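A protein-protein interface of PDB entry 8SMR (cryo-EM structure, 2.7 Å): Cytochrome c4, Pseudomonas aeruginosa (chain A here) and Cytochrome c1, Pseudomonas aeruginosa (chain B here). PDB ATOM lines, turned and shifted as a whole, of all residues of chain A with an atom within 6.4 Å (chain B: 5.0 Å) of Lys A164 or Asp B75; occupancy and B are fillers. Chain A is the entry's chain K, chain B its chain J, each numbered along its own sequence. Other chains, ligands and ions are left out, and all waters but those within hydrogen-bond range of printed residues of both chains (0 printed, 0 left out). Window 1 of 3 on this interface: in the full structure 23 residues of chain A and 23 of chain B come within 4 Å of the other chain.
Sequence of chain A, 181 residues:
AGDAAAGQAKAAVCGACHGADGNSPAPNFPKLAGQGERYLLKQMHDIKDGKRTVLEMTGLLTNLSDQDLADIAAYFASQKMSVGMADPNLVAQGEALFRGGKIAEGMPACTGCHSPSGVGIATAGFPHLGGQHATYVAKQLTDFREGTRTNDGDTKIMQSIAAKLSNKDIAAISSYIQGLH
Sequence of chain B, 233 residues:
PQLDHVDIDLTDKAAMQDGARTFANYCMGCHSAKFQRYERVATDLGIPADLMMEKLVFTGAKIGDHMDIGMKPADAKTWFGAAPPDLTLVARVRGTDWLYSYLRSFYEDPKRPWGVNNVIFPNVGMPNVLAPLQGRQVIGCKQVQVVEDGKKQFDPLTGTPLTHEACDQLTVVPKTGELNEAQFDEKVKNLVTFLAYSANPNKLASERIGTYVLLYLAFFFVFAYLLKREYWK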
ATOM      1  N   LYS A 102      13.091 -27.363  -9.884  1.00  0.00           N
ATOM      2  CA  LYS A 102      13.109 -28.809 -10.094  1.00  0.00           C
ATOM      3  C   LYS A 102      12.581 -29.476  -8.832  1.00  0.00           C
ATOM      4  O   LYS A 102      13.281 -29.518  -7.817  1.00  0.00           O
ATOM      5  CB  LYS A 102      14.515 -29.306 -10.421  1.00  0.00           C
ATOM      6  CG  LYS A 102      15.154 -28.666 -11.640  1.00  0.00           C
ATOM      7  CD  LYS A 102      16.603 -29.107 -11.771  1.00  0.00           C
ATOM      8  CE  LYS A 102      17.281 -28.488 -12.979  1.00  0.00           C
ATOM      9  NZ  LYS A 102      18.682 -28.971 -13.129  1.00  0.00           N
ATOM     10  N   GLU A 105      14.815 -32.784  -8.246  1.00  0.00           N
ATOM     11  CA  GLU A 105      16.150 -32.468  -7.757  1.00  0.00           C
ATOM     12  C   GLU A 105      16.133 -31.522  -6.565  1.00  0.00           C
ATOM     13  O   GLU A 105      17.194 -31.265  -5.985  1.00  0.00           O
ATOM     14  CB  GLU A 105      16.990 -31.854  -8.878  1.00  0.00           C
ATOM     15  CG  GLU A 105      17.549 -32.869  -9.860  1.00  0.00           C
ATOM     16  CD  GLU A 105      16.515 -33.349 -10.859  1.00  0.00           C
ATOM     17  OE1 GLU A 105      16.852 -34.214 -11.695  1.00  0.00           O
ATOM     18  OE2 GLU A 105      15.366 -32.862 -10.810  1.00  0.00           O
ATOM     19  N   GLY A 106      14.970 -31.007  -6.187  1.00  0.00           N
ATOM     20  CA  GLY A 106      14.883 -30.082  -5.072  1.00  0.00           C
ATOM     21  C   GLY A 106      15.553 -28.749  -5.325  1.00  0.00           C
ATOM     22  O   GLY A 106      16.110 -28.155  -4.394  1.00  0.00           O
ATOM     23  N   MET A 107      15.510 -28.261  -6.565  1.00  0.00           N
ATOM     24  CA  MET A 107      16.042 -26.939  -6.863  1.00  0.00           C
ATOM     25  C   MET A 107      14.923 -25.914  -6.802  1.00  0.00           C
ATOM     26  O   MET A 107      13.891 -26.104  -7.459  1.00  0.00           O
ATOM     27  CB  MET A 107      16.691 -26.907  -8.243  1.00  0.00           C
ATOM     28  CG  MET A 107      17.535 -25.663  -8.484  1.00  0.00           C
ATOM     29  SD  MET A 107      17.873 -25.355 -10.224  1.00  0.00           S
ATOM     30  CE  MET A 107      16.262 -24.813 -10.788  1.00  0.00           C
ATOM     31  N   PRO A 108      15.068 -24.827  -6.050  1.00  0.00           N
ATOM     32  CA  PRO A 108      13.982 -23.847  -5.975  1.00  0.00           C
ATOM     33  C   PRO A 108      13.761 -23.149  -7.304  1.00  0.00           C
ATOM     34  O   PRO A 108      14.665 -23.032  -8.134  1.00  0.00           O
ATOM     35  CB  PRO A 108      14.460 -22.853  -4.908  1.00  0.00           C
ATOM     36  CG  PRO A 108      15.706 -23.425  -4.330  1.00  0.00           C
ATOM     37  CD  PRO A 108      16.264 -24.362  -5.333  1.00  0.00           C
ATOM     38  N   ARG A 145      28.058 -22.317  -9.091  1.00  0.00           N
ATOM     39  CA  ARG A 145      28.075 -23.776  -9.115  1.00  0.00           C
ATOM     40  C   ARG A 145      29.451 -24.320  -8.754  1.00  0.00           C
ATOM     41  O   ARG A 145      29.564 -25.284  -7.989  1.00  0.00           O
ATOM     42  CB  ARG A 145      27.651 -24.272 -10.495  1.00  0.00           C
ATOM     43  CG  ARG A 145      27.504 -25.778 -10.600  1.00  0.00           C
ATOM     44  CD  ARG A 145      27.049 -26.186 -11.985  1.00  0.00           C
ATOM     45  NE  ARG A 145      28.065 -25.900 -12.988  1.00  0.00           N
ATOM     46  CZ  ARG A 145      27.857 -25.915 -14.297  1.00  0.00           C
ATOM     47  NH1 ARG A 145      26.671 -26.204 -14.805  1.00  0.00           N
ATOM     48  NH2 ARG A 145      28.864 -25.631 -15.116  1.00  0.00           N
ATOM     49  N   GLN A 159      25.232 -20.760  -4.263  1.00  0.00           N
ATOM     50  CA  GLN A 159      26.099 -21.905  -4.511  1.00  0.00           C
ATOM     51  C   GLN A 159      25.291 -23.196  -4.492  1.00  0.00           C
ATOM     52  O   GLN A 159      25.386 -24.020  -5.411  1.00  0.00           O
ATOM     53  CB  GLN A 159      27.222 -21.945  -3.477  1.00  0.00           C
ATOM     54  CG  GLN A 159      28.199 -20.791  -3.594  1.00  0.00           C
ATOM     55  CD  GLN A 159      29.284 -20.839  -2.543  1.00  0.00           C
ATOM     56  OE1 GLN A 159      30.123 -21.740  -2.543  1.00  0.00           O
ATOM     57  NE2 GLN A 159      29.278 -19.867  -1.641  1.00  0.00           N
ATOM     58  N   SER A 160      24.450 -23.363  -3.469  1.00  0.00           N
ATOM     59  CA  SER A 160      23.606 -24.549  -3.386  1.00  0.00           C
ATOM     60  C   SER A 160      22.631 -24.615  -4.554  1.00  0.00           C
ATOM     61  O   SER A 160      22.427 -25.683  -5.140  1.00  0.00           O
ATOM     62  CB  SER A 160      22.848 -24.555  -2.060  1.00  0.00           C
ATOM     63  OG  SER A 160      23.736 -24.473  -0.961  1.00  0.00           O
ATOM     64  N   ILE A 161      22.015 -23.485  -4.903  1.00  0.00           N
ATOM     65  CA  ILE A 161      21.022 -23.490  -5.975  1.00  0.00           C
ATOM     66  C   ILE A 161      21.672 -23.834  -7.312  1.00  0.00           C
ATOM     67  O   ILE A 161      21.146 -24.641  -8.085  1.00  0.00           O
ATOM     68  CB  ILE A 161      20.291 -22.138  -6.029  1.00  0.00           C
ATOM     69  CG1 ILE A 161      19.288 -22.044  -4.878  1.00  0.00           C
ATOM     70  CG2 ILE A 161      19.585 -21.962  -7.365  1.00  0.00           C
ATOM     71  CD1 ILE A 161      18.942 -20.638  -4.492  1.00  0.00           C
ATOM     72  N   ALA A 162      22.825 -23.227  -7.604  1.00  0.00           N
ATOM     73  CA  ALA A 162      23.504 -23.457  -8.871  1.00  0.00           C
ATOM     74  C   ALA A 162      24.161 -24.825  -8.935  1.00  0.00           C
ATOM     75  O   ALA A 162      24.429 -25.315 -10.037  1.00  0.00           O
ATOM     76  CB  ALA A 162      24.552 -22.370  -9.106  1.00  0.00           C
ATOM     77  N   ALA A 163      24.428 -25.455  -7.788  1.00  0.00           N
ATOM     78  CA  ALA A 163      24.927 -26.823  -7.809  1.00  0.00           C
ATOM     79  C   ALA A 163      23.974 -27.764  -8.532  1.00  0.00           C
ATOM     80  O   ALA A 163      24.410 -28.806  -9.033  1.00  0.00           O
ATOM     81  CB  ALA A 163      25.164 -27.320  -6.384  1.00  0.00           C
ATOM     82  N   LYS A 164      22.690 -27.422  -8.597  1.00  0.00           N
ATOM     83  CA  LYS A 164      21.671 -28.275  -9.191  1.00  0.00           C
ATOM     84  C   LYS A 164      21.382 -27.926 -10.648  1.00  0.00           C
ATOM     85  O   LYS A 164      20.500 -28.541 -11.255  1.00  0.00           O
ATOM     86  CB  LYS A 164      20.383 -28.189  -8.371  1.00  0.00           C
ATOM     87  CG  LYS A 164      20.614 -28.183  -6.866  1.00  0.00           C
ATOM     88  CD  LYS A 164      19.649 -29.096  -6.134  1.00  0.00           C
ATOM     89  CE  LYS A 164      20.095 -29.325  -4.701  1.00  0.00           C
ATOM     90  NZ  LYS A 164      18.976 -29.175  -3.731  1.00  0.00           N
ATOM     91  N   LEU A 165      22.100 -26.965 -11.224  1.00  0.00           N
ATOM     92  CA  LEU A 165      21.890 -26.542 -12.602  1.00  0.00           C
ATOM     93  C   LEU A 165      22.977 -27.124 -13.492  1.00  0.00           C
ATOM     94  O   LEU A 165      24.169 -26.976 -13.202  1.00  0.00           O
ATOM     95  CB  LEU A 165      21.892 -25.015 -12.719  1.00  0.00           C
ATOM     96  CG  LEU A 165      20.706 -24.268 -12.110  1.00  0.00           C
ATOM     97  CD1 LEU A 165      21.039 -22.794 -11.949  1.00  0.00           C
ATOM     98  CD2 LEU A 165      19.464 -24.446 -12.969  1.00  0.00           C
ATOM     99  N   SER A 166      22.563 -27.779 -14.571  1.00  0.00           N
ATOM    100  CA  SER A 166      23.499 -28.244 -15.579  1.00  0.00           C
ATOM    101  C   SER A 166      23.898 -27.088 -16.494  1.00  0.00           C
ATOM    102  O   SER A 166      23.345 -25.986 -16.428  1.00  0.00           O
ATOM    103  CB  SER A 166      22.889 -29.383 -16.394  1.00  0.00           C
ATOM    104  OG  SER A 166      21.918 -28.898 -17.304  1.00  0.00           O
ATOM    105  N   ASP A 169      20.986 -26.241 -18.552  1.00  0.00           N
ATOM    106  CA  ASP A 169      20.055 -25.497 -17.712  1.00  0.00           C
ATOM    107  C   ASP A 169      20.531 -24.069 -17.503  1.00  0.00           C
ATOM    108  O   ASP A 169      19.736 -23.126 -17.564  1.00  0.00           O
ATOM    109  CB  ASP A 169      19.883 -26.200 -16.365  1.00  0.00           C
ATOM    110  CG  ASP A 169      19.224 -27.557 -16.493  1.00  0.00           C
ATOM    111  OD1 ASP A 169      18.624 -27.833 -17.553  1.00  0.00           O
ATOM    112  OD2 ASP A 169      19.306 -28.349 -15.532  1.00  0.00           O
ATOM    113  N   LYS B  72      13.227 -26.991  -1.002  1.00  0.00           N
ATOM    114  CA  LYS B  72      13.070 -27.909   0.113  1.00  0.00           C
ATOM    115  C   LYS B  72      12.971 -27.141   1.432  1.00  0.00           C
ATOM    116  O   LYS B  72      13.591 -26.087   1.590  1.00  0.00           O
ATOM    117  CB  LYS B  72      14.242 -28.882   0.173  1.00  0.00           C
ATOM    118  CG  LYS B  72      14.413 -29.726  -1.080  1.00  0.00           C
ATOM    119  CD  LYS B  72      13.424 -30.883  -1.114  1.00  0.00           C
ATOM    120  CE  LYS B  72      13.896 -32.002  -2.027  1.00  0.00           C
ATOM    121  NZ  LYS B  72      12.810 -32.493  -2.920  1.00  0.00           N
ATOM    122  N   PRO B  73      12.188 -27.644   2.393  1.00  0.00           N
ATOM    123  CA  PRO B  73      12.071 -26.924   3.673  1.00  0.00           C
ATOM    124  C   PRO B  73      13.398 -26.718   4.384  1.00  0.00           C
ATOM    125  O   PRO B  73      13.611 -25.654   4.976  1.00  0.00           O
ATOM    126  CB  PRO B  73      11.121 -27.814   4.489  1.00  0.00           C
ATOM    127  CG  PRO B  73      10.380 -28.615   3.482  1.00  0.00           C
ATOM    128  CD  PRO B  73      11.331 -28.841   2.354  1.00  0.00           C
ATOM    129  N   ALA B  74      14.298 -27.703   4.354  1.00  0.00           N
ATOM    130  CA  ALA B  74      15.581 -27.544   5.032  1.00  0.00           C
ATOM    131  C   ALA B  74      16.438 -26.483   4.354  1.00  0.00           C
ATOM    132  O   ALA B  74      17.042 -25.636   5.026  1.00  0.00           O
ATOM    133  CB  ALA B  74      16.321 -28.881   5.073  1.00  0.00           C
ATOM    134  N   ASP B  75      16.502 -26.516   3.023  1.00  0.00           N
ATOM    135  CA  ASP B  75      17.250 -25.501   2.294  1.00  0.00           C
ATOM    136  C   ASP B  75      16.716 -24.108   2.595  1.00  0.00           C
ATOM    137  O   ASP B  75      17.487 -23.180   2.866  1.00  0.00           O
ATOM    138  CB  ASP B  75      17.180 -25.784   0.794  1.00  0.00           C
ATOM    139  CG  ASP B  75      18.231 -26.773   0.335  1.00  0.00           C
ATOM    140  OD1 ASP B  75      19.364 -26.731   0.856  1.00  0.00           O
ATOM    141  OD2 ASP B  75      17.923 -27.594  -0.554  1.00  0.00           O
ATOM    142  N   ALA B  76      15.393 -23.946   2.560  1.00  0.00           N
ATOM    143  CA  ALA B  76      14.804 -22.635   2.799  1.00  0.00           C
ATOM    144  C   ALA B  76      14.999 -22.193   4.243  1.00  0.00           C
ATOM    145  O   ALA B  76      15.161 -20.999   4.511  1.00  0.00           O
ATOM    146  CB  ALA B  76      13.321 -22.657   2.440  1.00  0.00           C
ATOM    147  N   LYS B  77      14.965 -23.132   5.190  1.00  0.00           N
ATOM    148  CA  LYS B  77      15.242 -22.776   6.578  1.00  0.00           C
ATOM    149  C   LYS B  77      16.671 -22.281   6.731  1.00  0.00           C
ATOM    150  O   LYS B  77      16.928 -21.304   7.444  1.00  0.00           O
ATOM    151  CB  LYS B  77      14.992 -23.973   7.494  1.00  0.00           C
ATOM    152  CG  LYS B  77      15.392 -23.726   8.939  1.00  0.00           C
ATOM    153  CD  LYS B  77      14.681 -24.681   9.892  1.00  0.00           C
ATOM    154  CE  LYS B  77      14.780 -24.245  11.354  1.00  0.00           C
ATOM    155  NZ  LYS B  77      14.875 -22.769  11.550  1.00  0.00           N
ATOM    156  N   THR B  78      17.619 -22.945   6.067  1.00  0.00           N
ATOM    157  CA  THR B  78      18.998 -22.472   6.089  1.00  0.00           C
ATOM    158  C   THR B  78      19.113 -21.084   5.472  1.00  0.00           C
ATOM    159  O   THR B  78      19.817 -20.216   6.001  1.00  0.00           O
ATOM    160  CB  THR B  78      19.902 -23.459   5.347  1.00  0.00           C
ATOM    161  OG1 THR B  78      19.982 -24.686   6.082  1.00  0.00           O
ATOM    162  CG2 THR B  78      21.299 -22.880   5.167  1.00  0.00           C
ATOM    163  N   TRP B  79      18.425 -20.856   4.354  1.00  0.00           N
ATOM    164  CA  TRP B  79      18.595 -19.614   3.607  1.00  0.00           C
ATOM    165  C   TRP B  79      17.922 -18.427   4.290  1.00  0.00           C
ATOM    166  O   TRP B  79      18.500 -17.336   4.349  1.00  0.00           O
ATOM    167  CB  TRP B  79      18.045 -19.787   2.192  1.00  0.00           C
ATOM    168  CG  TRP B  79      18.721 -20.876   1.423  1.00  0.00           C
ATOM    169  CD1 TRP B  79      19.973 -21.373   1.638  1.00  0.00           C
ATOM    170  CD2 TRP B  79      18.187 -21.600   0.312  1.00  0.00           C
ATOM    171  NE1 TRP B  79      20.250 -22.363   0.730  1.00  0.00           N
ATOM    172  CE2 TRP B  79      19.170 -22.522  -0.097  1.00  0.00           C
ATOM    173  CE3 TRP B  79      16.972 -21.559  -0.377  1.00  0.00           C
ATOM    174  CZ2 TRP B  79      18.975 -23.395  -1.162  1.00  0.00           C
ATOM    175  CZ3 TRP B  79      16.782 -22.426  -1.433  1.00  0.00           C
ATOM    176  CH2 TRP B  79      17.779 -23.331  -1.816  1.00  0.00           C
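Lys A164 touches just one residue of chain B: Asp B75. Asp B75 touches one residue of chain A. Printed residues of chain B within 4 Å of Gly A106: Lys B72. Printed residues of chain A within 4 Å of Trp B79: Pro A108 and Ile A161. Of the printed residues of chain A, Lys B72 touches Gly A106. Asp A169 touches none of the printed residues of chain B. Ala A163 touches none of the printed residues of chain B.
Among the printed residues, pairs that only touch across the chains: Pro A108 with Trp B79 (3.2 Å), Ile A161 with Trp B79 (3.6 Å) and Gly A106 with Lys B72 (3.7 Å).
The backbone carbonyl oxygen (O) of Lys A164 is in hydrogen-bond range of the side-chain amino group (NZ) of Lys A102. The backbone carbonyl oxygen of Gly A106 sits at hydrogen-bond distance from the side-chain amino group of Lys A164 (3.1 Å).
Hydrophobic or aromatic side chains of chain A within 4 Å of the printed part of chain B: Pro A108 and Ile A161. Among the printed residues, 4 pairs touch across the chains. Among the printed residues, Asp or Glu carboxylates within 4 Å of a Lys or Arg side-chain nitrogen of the other chain: Lys A164 with Asp B75 (3.7 Å).
OD2 of Asp B75 lies within salt-bridge range of NZ of Lys A164 (3.7 Å).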
